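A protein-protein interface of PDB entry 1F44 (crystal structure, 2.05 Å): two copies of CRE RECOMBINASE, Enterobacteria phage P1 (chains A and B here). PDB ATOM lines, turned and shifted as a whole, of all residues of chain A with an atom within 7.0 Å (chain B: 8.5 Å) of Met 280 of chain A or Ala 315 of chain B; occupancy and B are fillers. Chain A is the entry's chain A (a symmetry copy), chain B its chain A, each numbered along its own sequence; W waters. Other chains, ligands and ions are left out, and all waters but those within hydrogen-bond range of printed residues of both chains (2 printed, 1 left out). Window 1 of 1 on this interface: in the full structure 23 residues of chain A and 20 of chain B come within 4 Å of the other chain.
The backbone NH (N) of Thr 313 of chain B lies within hydrogen-bond range of the side-chain amide oxygen (OE1) of Gln 292 of chain A (2.7 Å).
The side-chain carboxylate (OE2) of Glu 289 of chain A is in salt-bridge range of the guanidinium group (NH2) of Arg 318 of chain B (3.2 Å).
SD of Met 280 of chain A sits close to SD of Met 316 of chain B (3.6 Å).
The side-chain carboxylate (OE2) of Glu 312 of chain B lies within hydrogen-bond range of the backbone NH (N) of Gly 314 of chain B (2.6 Å).
O of Thr 313 of chain B lies within hydrogen-bond range of NE of Arg 318 of chain B (3.0 Å).
O of Arg 318 of chain B sits at hydrogen-bond distance from N of Gly 323 of chain B.
The side-chain hydroxyl (OH) of Tyr 149 of chain A sits at hydrogen-bond distance from the side-chain carboxylate (OD2) of Asp 279 of chain A.
The guanidinium group (NH1) of Arg 273 of chain A is in hydrogen-bond range of the backbone carbonyl oxygen (O) of Leu 152 of chain A (2.7 Å).
O of Met 280 of chain A lies within hydrogen-bond range of N of Val 285 of chain A (3.2 Å).
CE of Met 316 of chain B touches CE2 of Tyr 149 of chain A (3.3 Å).
CD2 of Leu 320 of chain B touches CE2 of Tyr 149 of chain A, at 3.7 Å.
Met 316 of chain B touches Asn 150 of chain A (CB to O, 3.2 Å).
Leu 152 of chain A touches Met 316 of chain B.
Ala 315 of chain B touches Met 280 of chain A (CB to SD, 3.95 Å).
Met 280 of chain A touches Leu 319 of chain B (CG to CD1, 3.8 Å).
Leu 319 of chain B touches Ala 283 of chain A (CD2 to CB, 3.7 Å).
CG1 of Val 285 of chain A touches CB of Ala 315 of chain B, at 3.97 Å.
Glu 289 of chain A touches Thr 313 of chain B (CG to OG1, 3.7 Å).
Gln 292 of chain A touches Glu 312 of chain B.
Of the printed residues of chain B, Met 280 of chain A touches Ala 315 (3.95 Å), Met 316 (3.6 Å) and Leu 319 (3.8 Å).
Ala 281 of chain A touches none of the printed residues of chain B.
Printed residues of chain B within 4 Å of Ala 283 of chain A: Leu 319 (3.7 Å).
Of the printed residues of chain B, Tyr 149 of chain A touches Met 316 and Leu 320.
Of the printed residues of chain B, Gln 292 of chain A touches Glu 312 (3.7 Å) and Thr 313 (2.7 Å).
Gly 314 of chain B touches none of the printed residues of chain A.
Of the 12 printed residues of chain B, 7 touch a printed residue of chain A.
Hydrophobic or aromatic side chains of chain B that line the printed part of chain A: Ala 315, Met 316, Leu 319 and Leu 320.
Of the 25 printed residues of chain A, 9 touch a printed residue of chain B.
Among the printed residues, Asp or Glu carboxylates within 4 Å of a Lys or Arg side-chain nitrogen of the other chain: Glu 289 of chain A with Arg 318 of chain B.
No position is printed for both chains.
Water W2 lies within hydrogen-bond range of OE2 of Glu 312 of chain B and N of Ala 293 of chain A.
Water W1 lies within hydrogen-bond range of the side-chain hydroxyl of Thr 313 of chain B (2.6 Å), the backbone carbonyl oxygen of Glu 289 of chain A (2.7 Å) and the backbone NH of Ala 315 of chain B (3.1 Å).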
ATOM      1  N   TYR A 149     -14.442  25.850 -38.843  1.00  0.00           N
ATOM      2  CA  TYR A 149     -14.285  24.773 -37.889  1.00  0.00           C
ATOM      3  C   TYR A 149     -13.617  25.233 -36.576  1.00  0.00           C
ATOM      4  O   TYR A 149     -14.074  24.877 -35.484  1.00  0.00           O
ATOM      5  CB  TYR A 149     -13.535  23.600 -38.493  1.00  0.00           C
ATOM      6  CG  TYR A 149     -13.309  22.488 -37.499  1.00  0.00           C
ATOM      7  CD1 TYR A 149     -14.344  21.599 -37.172  1.00  0.00           C
ATOM      8  CD2 TYR A 149     -12.089  22.344 -36.848  1.00  0.00           C
ATOM      9  CE1 TYR A 149     -14.166  20.573 -36.215  1.00  0.00           C
ATOM     10  CE2 TYR A 149     -11.881  21.314 -35.897  1.00  0.00           C
ATOM     11  CZ  TYR A 149     -12.927  20.449 -35.581  1.00  0.00           C
ATOM     12  OH  TYR A 149     -12.757  19.493 -34.619  1.00  0.00           O
ATOM     13  N   ASN A 150     -12.545  26.020 -36.707  1.00  0.00           N
ATOM     14  CA  ASN A 150     -11.752  26.544 -35.574  1.00  0.00           C
ATOM     15  C   ASN A 150     -12.531  27.540 -34.720  1.00  0.00           C
ATOM     16  O   ASN A 150     -12.426  27.543 -33.495  1.00  0.00           O
ATOM     17  CB  ASN A 150     -10.521  27.255 -36.165  1.00  0.00           C
ATOM     18  CG  ASN A 150      -9.398  27.546 -35.154  1.00  0.00           C
ATOM     19  OD1 ASN A 150      -8.274  27.698 -35.587  1.00  0.00           O
ATOM     20  ND2 ASN A 150      -9.703  27.699 -33.853  1.00  0.00           N
ATOM     21  N   LEU A 152     -16.072  28.254 -35.116  1.00  0.00           N
ATOM     22  CA  LEU A 152     -17.506  27.969 -34.942  1.00  0.00           C
ATOM     23  C   LEU A 152     -18.355  29.189 -35.314  1.00  0.00           C
ATOM     24  O   LEU A 152     -19.540  29.268 -35.003  1.00  0.00           O
ATOM     25  CB  LEU A 152     -17.812  27.551 -33.469  1.00  0.00           C
ATOM     26  CG  LEU A 152     -17.445  26.121 -33.049  1.00  0.00           C
ATOM     27  CD1 LEU A 152     -15.994  26.058 -32.561  1.00  0.00           C
ATOM     28  CD2 LEU A 152     -18.401  25.695 -31.948  1.00  0.00           C
ATOM     29  N   ARG A 273     -19.786  24.334 -37.307  1.00  0.00           N
ATOM     30  CA  ARG A 273     -20.164  24.703 -35.945  1.00  0.00           C
ATOM     31  C   ARG A 273     -20.741  23.432 -35.238  1.00  0.00           C
ATOM     32  O   ARG A 273     -20.326  23.075 -34.105  1.00  0.00           O
ATOM     33  CB  ARG A 273     -21.190  25.835 -35.968  1.00  0.00           C
ATOM     34  CG  ARG A 273     -21.674  26.276 -34.573  1.00  0.00           C
ATOM     35  CD  ARG A 273     -22.456  27.570 -34.675  1.00  0.00           C
ATOM     36  NE  ARG A 273     -23.031  28.018 -33.407  1.00  0.00           N
ATOM     37  CZ  ARG A 273     -22.415  28.841 -32.564  1.00  0.00           C
ATOM     38  NH1 ARG A 273     -21.185  29.276 -32.819  1.00  0.00           N
ATOM     39  NH2 ARG A 273     -23.025  29.230 -31.452  1.00  0.00           N
ATOM     40  N   GLY A 275     -20.174  20.311 -36.124  1.00  0.00           N
ATOM     41  CA  GLY A 275     -19.065  19.384 -36.003  1.00  0.00           C
ATOM     42  C   GLY A 275     -18.077  19.684 -34.890  1.00  0.00           C
ATOM     43  O   GLY A 275     -17.693  18.788 -34.123  1.00  0.00           O
ATOM     44  N   ALA A 276     -17.613  20.928 -34.812  1.00  0.00           N
ATOM     45  CA  ALA A 276     -16.647  21.300 -33.771  1.00  0.00           C
ATOM     46  C   ALA A 276     -17.252  21.154 -32.356  1.00  0.00           C
ATOM     47  O   ALA A 276     -16.551  20.809 -31.423  1.00  0.00           O
ATOM     48  CB  ALA A 276     -16.151  22.725 -33.985  1.00  0.00           C
ATOM     49  N   ALA A 277     -18.546  21.462 -32.216  1.00  0.00           N
ATOM     50  CA  ALA A 277     -19.232  21.373 -30.908  1.00  0.00           C
ATOM     51  C   ALA A 277     -19.260  19.918 -30.460  1.00  0.00           C
ATOM     52  O   ALA A 277     -18.970  19.609 -29.306  1.00  0.00           O
ATOM     53  CB  ALA A 277     -20.627  21.946 -30.997  1.00  0.00           C
ATOM     54  N   ARG A 278     -19.550  19.010 -31.392  1.00  0.00           N
ATOM     55  CA  ARG A 278     -19.529  17.580 -31.093  1.00  0.00           C
ATOM     56  C   ARG A 278     -18.107  17.124 -30.752  1.00  0.00           C
ATOM     57  O   ARG A 278     -17.891  16.339 -29.834  1.00  0.00           O
ATOM     58  CB  ARG A 278     -20.069  16.787 -32.289  1.00  0.00           C
ATOM     59  CG  ARG A 278     -21.586  16.958 -32.491  1.00  0.00           C
ATOM     60  CD  ARG A 278     -22.182  15.868 -33.444  1.00  0.00           C
ATOM     61  NE  ARG A 278     -23.461  16.299 -34.003  1.00  0.00           N
ATOM     62  CZ  ARG A 278     -23.961  15.865 -35.158  1.00  0.00           C
ATOM     63  NH1 ARG A 278     -23.316  14.949 -35.864  1.00  0.00           N
ATOM     64  NH2 ARG A 278     -25.121  16.334 -35.597  1.00  0.00           N
ATOM     65  N   ASP A 279     -17.123  17.621 -31.476  1.00  0.00           N
ATOM     66  CA  ASP A 279     -15.732  17.221 -31.182  1.00  0.00           C
ATOM     67  C   ASP A 279     -15.281  17.632 -29.786  1.00  0.00           C
ATOM     68  O   ASP A 279     -14.567  16.878 -29.113  1.00  0.00           O
ATOM     69  CB  ASP A 279     -14.739  17.760 -32.215  1.00  0.00           C
ATOM     70  CG  ASP A 279     -14.819  17.016 -33.560  1.00  0.00           C
ATOM     71  OD1 ASP A 279     -15.293  15.841 -33.575  1.00  0.00           O
ATOM     72  OD2 ASP A 279     -14.448  17.639 -34.593  1.00  0.00           O
ATOM     73  N   MET A 280     -15.672  18.834 -29.366  1.00  0.00           N
ATOM     74  CA  MET A 280     -15.309  19.334 -28.032  1.00  0.00           C
ATOM     75  C   MET A 280     -16.032  18.503 -26.977  1.00  0.00           C
ATOM     76  O   MET A 280     -15.442  18.052 -26.015  1.00  0.00           O
ATOM     77  CB  MET A 280     -15.669  20.820 -27.889  1.00  0.00           C
ATOM     78  CG  MET A 280     -14.576  21.777 -28.436  1.00  0.00           C
ATOM     79  SD  MET A 280     -14.999  23.491 -28.231  1.00  0.00           S
ATOM     80  CE  MET A 280     -16.519  23.633 -29.195  1.00  0.00           C
ATOM     81  N   ALA A 281     -17.318  18.281 -27.176  1.00  0.00           N
ATOM     82  CA  ALA A 281     -18.051  17.453 -26.238  1.00  0.00           C
ATOM     83  C   ALA A 281     -17.382  16.084 -26.176  1.00  0.00           C
ATOM     84  O   ALA A 281     -17.124  15.582 -25.101  1.00  0.00           O
ATOM     85  CB  ALA A 281     -19.534  17.317 -26.651  1.00  0.00           C
ATOM     86  N   ARG A 282     -17.075  15.484 -27.323  1.00  0.00           N
ATOM     87  CA  ARG A 282     -16.477  14.133 -27.332  1.00  0.00           C
ATOM     88  C   ARG A 282     -15.116  14.030 -26.678  1.00  0.00           C
ATOM     89  O   ARG A 282     -14.769  12.994 -26.131  1.00  0.00           O
ATOM     90  CB  ARG A 282     -16.481  13.503 -28.748  1.00  0.00           C
ATOM     91  CG  ARG A 282     -15.165  13.559 -29.496  1.00  0.00           C
ATOM     92  CD  ARG A 282     -15.222  12.781 -30.852  1.00  0.00           C
ATOM     93  NE  ARG A 282     -15.843  13.578 -31.904  1.00  0.00           N
ATOM     94  CZ  ARG A 282     -17.114  13.450 -32.280  1.00  0.00           C
ATOM     95  NH1 ARG A 282     -17.860  12.508 -31.718  1.00  0.00           N
ATOM     96  NH2 ARG A 282     -17.634  14.246 -33.225  1.00  0.00           N
ATOM     97  N   ALA A 283     -14.373  15.136 -26.695  1.00  0.00           N
ATOM     98  CA  ALA A 283     -13.029  15.204 -26.104  1.00  0.00           C
ATOM     99  C   ALA A 283     -13.043  15.497 -24.586  1.00  0.00           C
ATOM    100  O   ALA A 283     -12.011  15.714 -23.981  1.00  0.00           O
ATOM    101  CB  ALA A 283     -12.151  16.252 -26.874  1.00  0.00           C
ATOM    102  N   GLY A 284     -14.217  15.542 -23.983  1.00  0.00           N
ATOM    103  CA  GLY A 284     -14.291  15.806 -22.557  1.00  0.00           C
ATOM    104  C   GLY A 284     -14.111  17.293 -22.185  1.00  0.00           C
ATOM    105  O   GLY A 284     -13.978  17.637 -21.028  1.00  0.00           O
ATOM    106  N   VAL A 285     -14.134  18.188 -23.150  1.00  0.00           N
ATOM    107  CA  VAL A 285     -14.029  19.614 -22.820  1.00  0.00           C
ATOM    108  C   VAL A 285     -15.239  20.046 -21.939  1.00  0.00           C
ATOM    109  O   VAL A 285     -16.396  19.614 -22.140  1.00  0.00           O
ATOM    110  CB  VAL A 285     -14.005  20.460 -24.111  1.00  0.00           C
ATOM    111  CG1 VAL A 285     -13.992  21.950 -23.795  1.00  0.00           C
ATOM    112  CG2 VAL A 285     -12.809  20.061 -24.988  1.00  0.00           C
ATOM    113  N   SER A 286     -14.960  20.888 -20.956  1.00  0.00           N
ATOM    114  CA  SER A 286     -16.005  21.366 -20.060  1.00  0.00           C
ATOM    115  C   SER A 286     -17.004  22.277 -20.764  1.00  0.00           C
ATOM    116  O   SER A 286     -16.716  22.894 -21.801  1.00  0.00           O
ATOM    117  CB  SER A 286     -15.407  22.092 -18.838  1.00  0.00           C
ATOM    118  OG  SER A 286     -14.910  23.377 -19.179  1.00  0.00           O
ATOM    119  N   GLU A 289     -15.919  26.084 -21.325  1.00  0.00           N
ATOM    120  CA  GLU A 289     -14.962  26.207 -22.416  1.00  0.00           C
ATOM    121  C   GLU A 289     -15.638  25.953 -23.772  1.00  0.00           C
ATOM    122  O   GLU A 289     -15.287  26.591 -24.751  1.00  0.00           O
ATOM    123  CB  GLU A 289     -13.768  25.291 -22.199  1.00  0.00           C
ATOM    124  CG  GLU A 289     -13.021  25.635 -20.928  1.00  0.00           C
ATOM    125  CD  GLU A 289     -11.674  24.931 -20.860  1.00  0.00           C
ATOM    126  OE1 GLU A 289     -11.406  24.138 -21.770  1.00  0.00           O
ATOM    127  OE2 GLU A 289     -10.878  25.184 -19.928  1.00  0.00           O
ATOM    128  N   ILE A 290     -16.630  25.054 -23.814  1.00  0.00           N
ATOM    129  CA  ILE A 290     -17.377  24.803 -25.068  1.00  0.00           C
ATOM    130  C   ILE A 290     -18.203  26.060 -25.342  1.00  0.00           C
ATOM    131  O   ILE A 290     -18.294  26.520 -26.472  1.00  0.00           O
ATOM    132  CB  ILE A 290     -18.371  23.557 -24.980  1.00  0.00           C
ATOM    133  CG1 ILE A 290     -17.603  22.247 -24.896  1.00  0.00           C
ATOM    134  CG2 ILE A 290     -19.340  23.524 -26.192  1.00  0.00           C
ATOM    135  CD1 ILE A 290     -18.529  21.018 -24.658  1.00  0.00           C
ATOM    136  N   MET A 291     -18.780  26.640 -24.297  1.00  0.00           N
ATOM    137  CA  MET A 291     -19.590  27.827 -24.473  1.00  0.00           C
ATOM    138  C   MET A 291     -18.759  28.986 -25.014  1.00  0.00           C
ATOM    139  O   MET A 291     -19.177  29.715 -25.930  1.00  0.00           O
ATOM    140  CB  MET A 291     -20.293  28.192 -23.159  1.00  0.00           C
ATOM    141  CG  MET A 291     -21.240  27.101 -22.691  1.00  0.00           C
ATOM    142  SD  MET A 291     -22.239  27.447 -21.207  1.00  0.00           S
ATOM    143  CE  MET A 291     -23.256  28.825 -21.765  1.00  0.00           C
ATOM    144  N   GLN A 292     -17.554  29.140 -24.472  1.00  0.00           N
ATOM    145  CA  GLN A 292     -16.667  30.204 -24.946  1.00  0.00           C
ATOM    146  C   GLN A 292     -16.245  29.986 -26.407  1.00  0.00           C
ATOM    147  O   GLN A 292     -16.192  30.931 -27.197  1.00  0.00           O
ATOM    148  CB  GLN A 292     -15.426  30.339 -24.066  1.00  0.00           C
ATOM    149  CG  GLN A 292     -14.682  31.629 -24.367  1.00  0.00           C
ATOM    150  CD  GLN A 292     -13.445  31.845 -23.494  1.00  0.00           C
ATOM    151  OE1 GLN A 292     -12.541  30.990 -23.425  1.00  0.00           O
ATOM    152  NE2 GLN A 292     -13.363  33.020 -22.887  1.00  0.00           N
ATOM    153  N   ALA A 293     -15.978  28.732 -26.765  1.00  0.00           N
ATOM    154  CA  ALA A 293     -15.568  28.378 -28.125  1.00  0.00           C
ATOM    155  C   ALA A 293     -16.593  28.775 -29.186  1.00  0.00           C
ATOM    156  O   ALA A 293     -16.221  29.161 -30.287  1.00  0.00           O
ATOM    157  CB  ALA A 293     -15.235  26.890 -28.223  1.00  0.00           C
ATOM    158  N   GLY A 294     -17.876  28.681 -28.854  1.00  0.00           N
ATOM    159  CA  GLY A 294     -18.928  29.015 -29.798  1.00  0.00           C
ATOM    160  C   GLY A 294     -19.737  30.253 -29.455  1.00  0.00           C
ATOM    161  O   GLY A 294     -20.722  30.553 -30.113  1.00  0.00           O
ATOM    162  N   TRP A 296     -21.656  30.815 -26.740  1.00  0.00           N
ATOM    163  CA  TRP A 296     -22.952  30.620 -26.075  1.00  0.00           C
ATOM    164  C   TRP A 296     -22.938  31.229 -24.657  1.00  0.00           C
ATOM    165  O   TRP A 296     -21.925  31.202 -23.985  1.00  0.00           O
ATOM    166  CB  TRP A 296     -23.234  29.115 -25.940  1.00  0.00           C
ATOM    167  CG  TRP A 296     -23.622  28.400 -27.247  1.00  0.00           C
ATOM    168  CD1 TRP A 296     -24.892  28.332 -27.811  1.00  0.00           C
ATOM    169  CD2 TRP A 296     -22.784  27.551 -28.060  1.00  0.00           C
ATOM    170  NE1 TRP A 296     -24.871  27.533 -28.937  1.00  0.00           N
ATOM    171  CE2 TRP A 296     -23.615  27.001 -29.088  1.00  0.00           C
ATOM    172  CE3 TRP A 296     -21.436  27.171 -28.006  1.00  0.00           C
ATOM    173  CZ2 TRP A 296     -23.109  26.149 -30.090  1.00  0.00           C
ATOM    174  CZ3 TRP A 296     -20.945  26.285 -28.988  1.00  0.00           C
ATOM    175  CH2 TRP A 296     -21.779  25.805 -30.022  1.00  0.00           C
ATOM    176  N   ILE A 306     -25.757  20.462 -29.010  1.00  0.00           N
ATOM    177  CA  ILE A 306     -24.938  19.267 -29.037  1.00  0.00           C
ATOM    178  C   ILE A 306     -25.736  18.009 -28.688  1.00  0.00           C
ATOM    179  O   ILE A 306     -25.192  17.055 -28.176  1.00  0.00           O
ATOM    180  CB  ILE A 306     -23.722  19.429 -28.118  1.00  0.00           C
ATOM    181  CG1 ILE A 306     -23.017  20.732 -28.477  1.00  0.00           C
ATOM    182  CG2 ILE A 306     -22.738  18.356 -28.378  1.00  0.00           C
ATOM    183  CD1 ILE A 306     -21.549  20.725 -28.177  1.00  0.00           C
ATOM    184  N   LEU A 309     -24.406  14.221 -30.106  1.00  0.00           N
ATOM    185  CA  LEU A 309     -23.027  13.743 -29.873  1.00  0.00           C
ATOM    186  C   LEU A 309     -22.980  12.364 -30.563  1.00  0.00           C
ATOM    187  O   LEU A 309     -23.811  11.513 -30.292  1.00  0.00           O
ATOM    188  CB  LEU A 309     -22.728  13.616 -28.364  1.00  0.00           C
ATOM    189  CG  LEU A 309     -21.426  12.900 -27.981  1.00  0.00           C
ATOM    190  CD1 LEU A 309     -20.294  13.523 -28.813  1.00  0.00           C
ATOM    191  CD2 LEU A 309     -21.151  13.040 -26.443  1.00  0.00           C
ATOM    192  N   GLU B 312      -8.929  33.776 -22.611  1.00  0.00           N
ATOM    193  CA  GLU B 312      -9.300  32.891 -23.701  1.00  0.00           C
ATOM    194  C   GLU B 312      -8.908  31.488 -23.377  1.00  0.00           C
ATOM    195  O   GLU B 312      -7.726  31.222 -23.199  1.00  0.00           O
ATOM    196  CB  GLU B 312      -8.511  33.289 -24.946  1.00  0.00           C
ATOM    197  CG  GLU B 312      -8.703  32.348 -26.118  1.00  0.00           C
ATOM    198  CD  GLU B 312     -10.163  32.084 -26.391  1.00  0.00           C
ATOM    199  OE1 GLU B 312     -10.932  33.060 -26.503  1.00  0.00           O
ATOM    200  OE2 GLU B 312     -10.542  30.906 -26.488  1.00  0.00           O
ATOM    201  N   THR B 313      -9.856  30.560 -23.344  1.00  0.00           N
ATOM    202  CA  THR B 313      -9.460  29.171 -23.035  1.00  0.00           C
ATOM    203  C   THR B 313      -8.998  28.360 -24.263  1.00  0.00           C
ATOM    204  O   THR B 313      -8.415  27.302 -24.130  1.00  0.00           O
ATOM    205  CB  THR B 313     -10.538  28.393 -22.225  1.00  0.00           C
ATOM    206  OG1 THR B 313     -11.768  28.404 -22.958  1.00  0.00           O
ATOM    207  CG2 THR B 313     -10.757  29.039 -20.832  1.00  0.00           C
ATOM    208  N   GLY B 314      -9.256  28.868 -25.455  1.00  0.00           N
ATOM    209  CA  GLY B 314      -8.810  28.225 -26.688  1.00  0.00           C
ATOM    210  C   GLY B 314      -8.998  26.718 -26.750  1.00  0.00           C
ATOM    211  O   GLY B 314      -8.098  25.993 -27.168  1.00  0.00           O
ATOM    212  N   ALA B 315     -10.202  26.241 -26.440  1.00  0.00           N
ATOM    213  CA  ALA B 315     -10.469  24.807 -26.574  1.00  0.00           C
ATOM    214  C   ALA B 315     -10.264  24.281 -28.027  1.00  0.00           C
ATOM    215  O   ALA B 315      -9.733  23.196 -28.215  1.00  0.00           O
ATOM    216  CB  ALA B 315     -11.863  24.447 -26.027  1.00  0.00           C
ATOM    217  N   MET B 316     -10.678  25.048 -29.041  1.00  0.00           N
ATOM    218  CA  MET B 316     -10.487  24.603 -30.424  1.00  0.00           C
ATOM    219  C   MET B 316      -9.005  24.621 -30.839  1.00  0.00           C
ATOM    220  O   MET B 316      -8.528  23.704 -31.516  1.00  0.00           O
ATOM    221  CB  MET B 316     -11.352  25.392 -31.396  1.00  0.00           C
ATOM    222  CG  MET B 316     -12.814  25.085 -31.278  1.00  0.00           C
ATOM    223  SD  MET B 316     -13.228  23.279 -31.413  1.00  0.00           S
ATOM    224  CE  MET B 316     -12.673  22.917 -33.099  1.00  0.00           C
ATOM    225  N   VAL B 317      -8.249  25.632 -30.405  1.00  0.00           N
ATOM    226  CA  VAL B 317      -6.810  25.662 -30.728  1.00  0.00           C
ATOM    227  C   VAL B 317      -6.185  24.415 -30.103  1.00  0.00           C
ATOM    228  O   VAL B 317      -5.460  23.689 -30.770  1.00  0.00           O
ATOM    229  CB  VAL B 317      -6.075  26.976 -30.190  1.00  0.00           C
ATOM    230  CG1 VAL B 317      -4.542  26.794 -30.156  1.00  0.00           C
ATOM    231  CG2 VAL B 317      -6.447  28.185 -31.023  1.00  0.00           C
ATOM    232  N   ARG B 318      -6.504  24.118 -28.843  1.00  0.00           N
ATOM    233  CA  ARG B 318      -5.910  22.947 -28.205  1.00  0.00           C
ATOM    234  C   ARG B 318      -6.242  21.652 -28.925  1.00  0.00           C
ATOM    235  O   ARG B 318      -5.382  20.803 -29.158  1.00  0.00           O
ATOM    236  CB  ARG B 318      -6.301  22.847 -26.730  1.00  0.00           C
ATOM    237  CG  ARG B 318      -6.085  24.129 -25.905  1.00  0.00           C
ATOM    238  CD  ARG B 318      -6.199  23.816 -24.385  1.00  0.00           C
ATOM    239  NE  ARG B 318      -7.288  24.541 -23.735  1.00  0.00           N
ATOM    240  CZ  ARG B 318      -8.387  23.979 -23.259  1.00  0.00           C
ATOM    241  NH1 ARG B 318      -8.570  22.670 -23.358  1.00  0.00           N
ATOM    242  NH2 ARG B 318      -9.323  24.739 -22.708  1.00  0.00           N
ATOM    243  N   LEU B 319      -7.499  21.490 -29.297  1.00  0.00           N
ATOM    244  CA  LEU B 319      -7.897  20.278 -30.030  1.00  0.00           C
ATOM    245  C   LEU B 319      -7.126  20.168 -31.368  1.00  0.00           C
ATOM    246  O   LEU B 319      -6.620  19.105 -31.716  1.00  0.00           O
ATOM    247  CB  LEU B 319      -9.411  20.332 -30.344  1.00  0.00           C
ATOM    248  CG  LEU B 319     -10.426  19.758 -29.365  1.00  0.00           C
ATOM    249  CD1 LEU B 319     -11.769  19.723 -30.034  1.00  0.00           C
ATOM    250  CD2 LEU B 319      -9.995  18.371 -28.967  1.00  0.00           C
ATOM    251  N   LEU B 320      -7.104  21.257 -32.138  1.00  0.00           N
ATOM    252  CA  LEU B 320      -6.453  21.278 -33.457  1.00  0.00           C
ATOM    253  C   LEU B 320      -4.943  21.042 -33.369  1.00  0.00           C
ATOM    254  O   LEU B 320      -4.334  20.383 -34.220  1.00  0.00           O
ATOM    255  CB  LEU B 320      -6.763  22.612 -34.166  1.00  0.00           C
ATOM    256  CG  LEU B 320      -8.160  22.759 -34.806  1.00  0.00           C
ATOM    257  CD1 LEU B 320      -8.522  24.195 -35.082  1.00  0.00           C
ATOM    258  CD2 LEU B 320      -8.231  21.935 -36.090  1.00  0.00           C
ATOM    259  N   GLU B 321      -4.340  21.585 -32.327  1.00  0.00           N
ATOM    260  CA  GLU B 321      -2.922  21.414 -32.138  1.00  0.00           C
ATOM    261  C   GLU B 321      -2.708  20.117 -31.339  1.00  0.00           C
ATOM    262  O   GLU B 321      -1.582  19.745 -31.057  1.00  0.00           O
ATOM    263  CB  GLU B 321      -2.317  22.678 -31.478  1.00  0.00           C
ATOM    264  CG  GLU B 321      -2.421  23.932 -32.427  1.00  0.00           C
ATOM    265  CD  GLU B 321      -1.844  25.217 -31.849  1.00  0.00           C
ATOM    266  OE1 GLU B 321      -1.106  25.165 -30.855  1.00  0.00           O
ATOM    267  OE2 GLU B 321      -2.115  26.296 -32.400  1.00  0.00           O
ATOM    268  N   ASP B 322      -3.834  19.428 -31.069  1.00  0.00           N
ATOM    269  CA  ASP B 322      -3.974  18.149 -30.301  1.00  0.00           C
ATOM    270  C   ASP B 322      -3.355  18.272 -28.943  1.00  0.00           C
ATOM    271  O   ASP B 322      -2.234  17.810 -28.719  1.00  0.00           O
ATOM    272  CB  ASP B 322      -3.431  16.946 -31.063  1.00  0.00           C
ATOM    273  CG  ASP B 322      -4.310  16.561 -32.236  1.00  0.00           C
ATOM    274  OD1 ASP B 322      -4.142  17.156 -33.313  1.00  0.00           O
ATOM    275  OD2 ASP B 322      -5.187  15.687 -32.074  1.00  0.00           O
ATOM    276  N   GLY B 323      -4.041  18.988 -28.056  1.00  0.00           N
ATOM    277  CA  GLY B 323      -3.465  19.355 -26.779  1.00  0.00           C
ATOM    278  C   GLY B 323      -2.445  20.296 -27.413  1.00  0.00           C
ATOM    279  O   GLY B 323      -2.725  21.470 -27.664  1.00  0.00           O
HETATM  280  O   HOH W   1     -12.738  27.484 -25.186  1.00  0.00           O
HETATM  281  O   HOH W   2     -12.638  29.685 -27.026  1.00  0.00           O
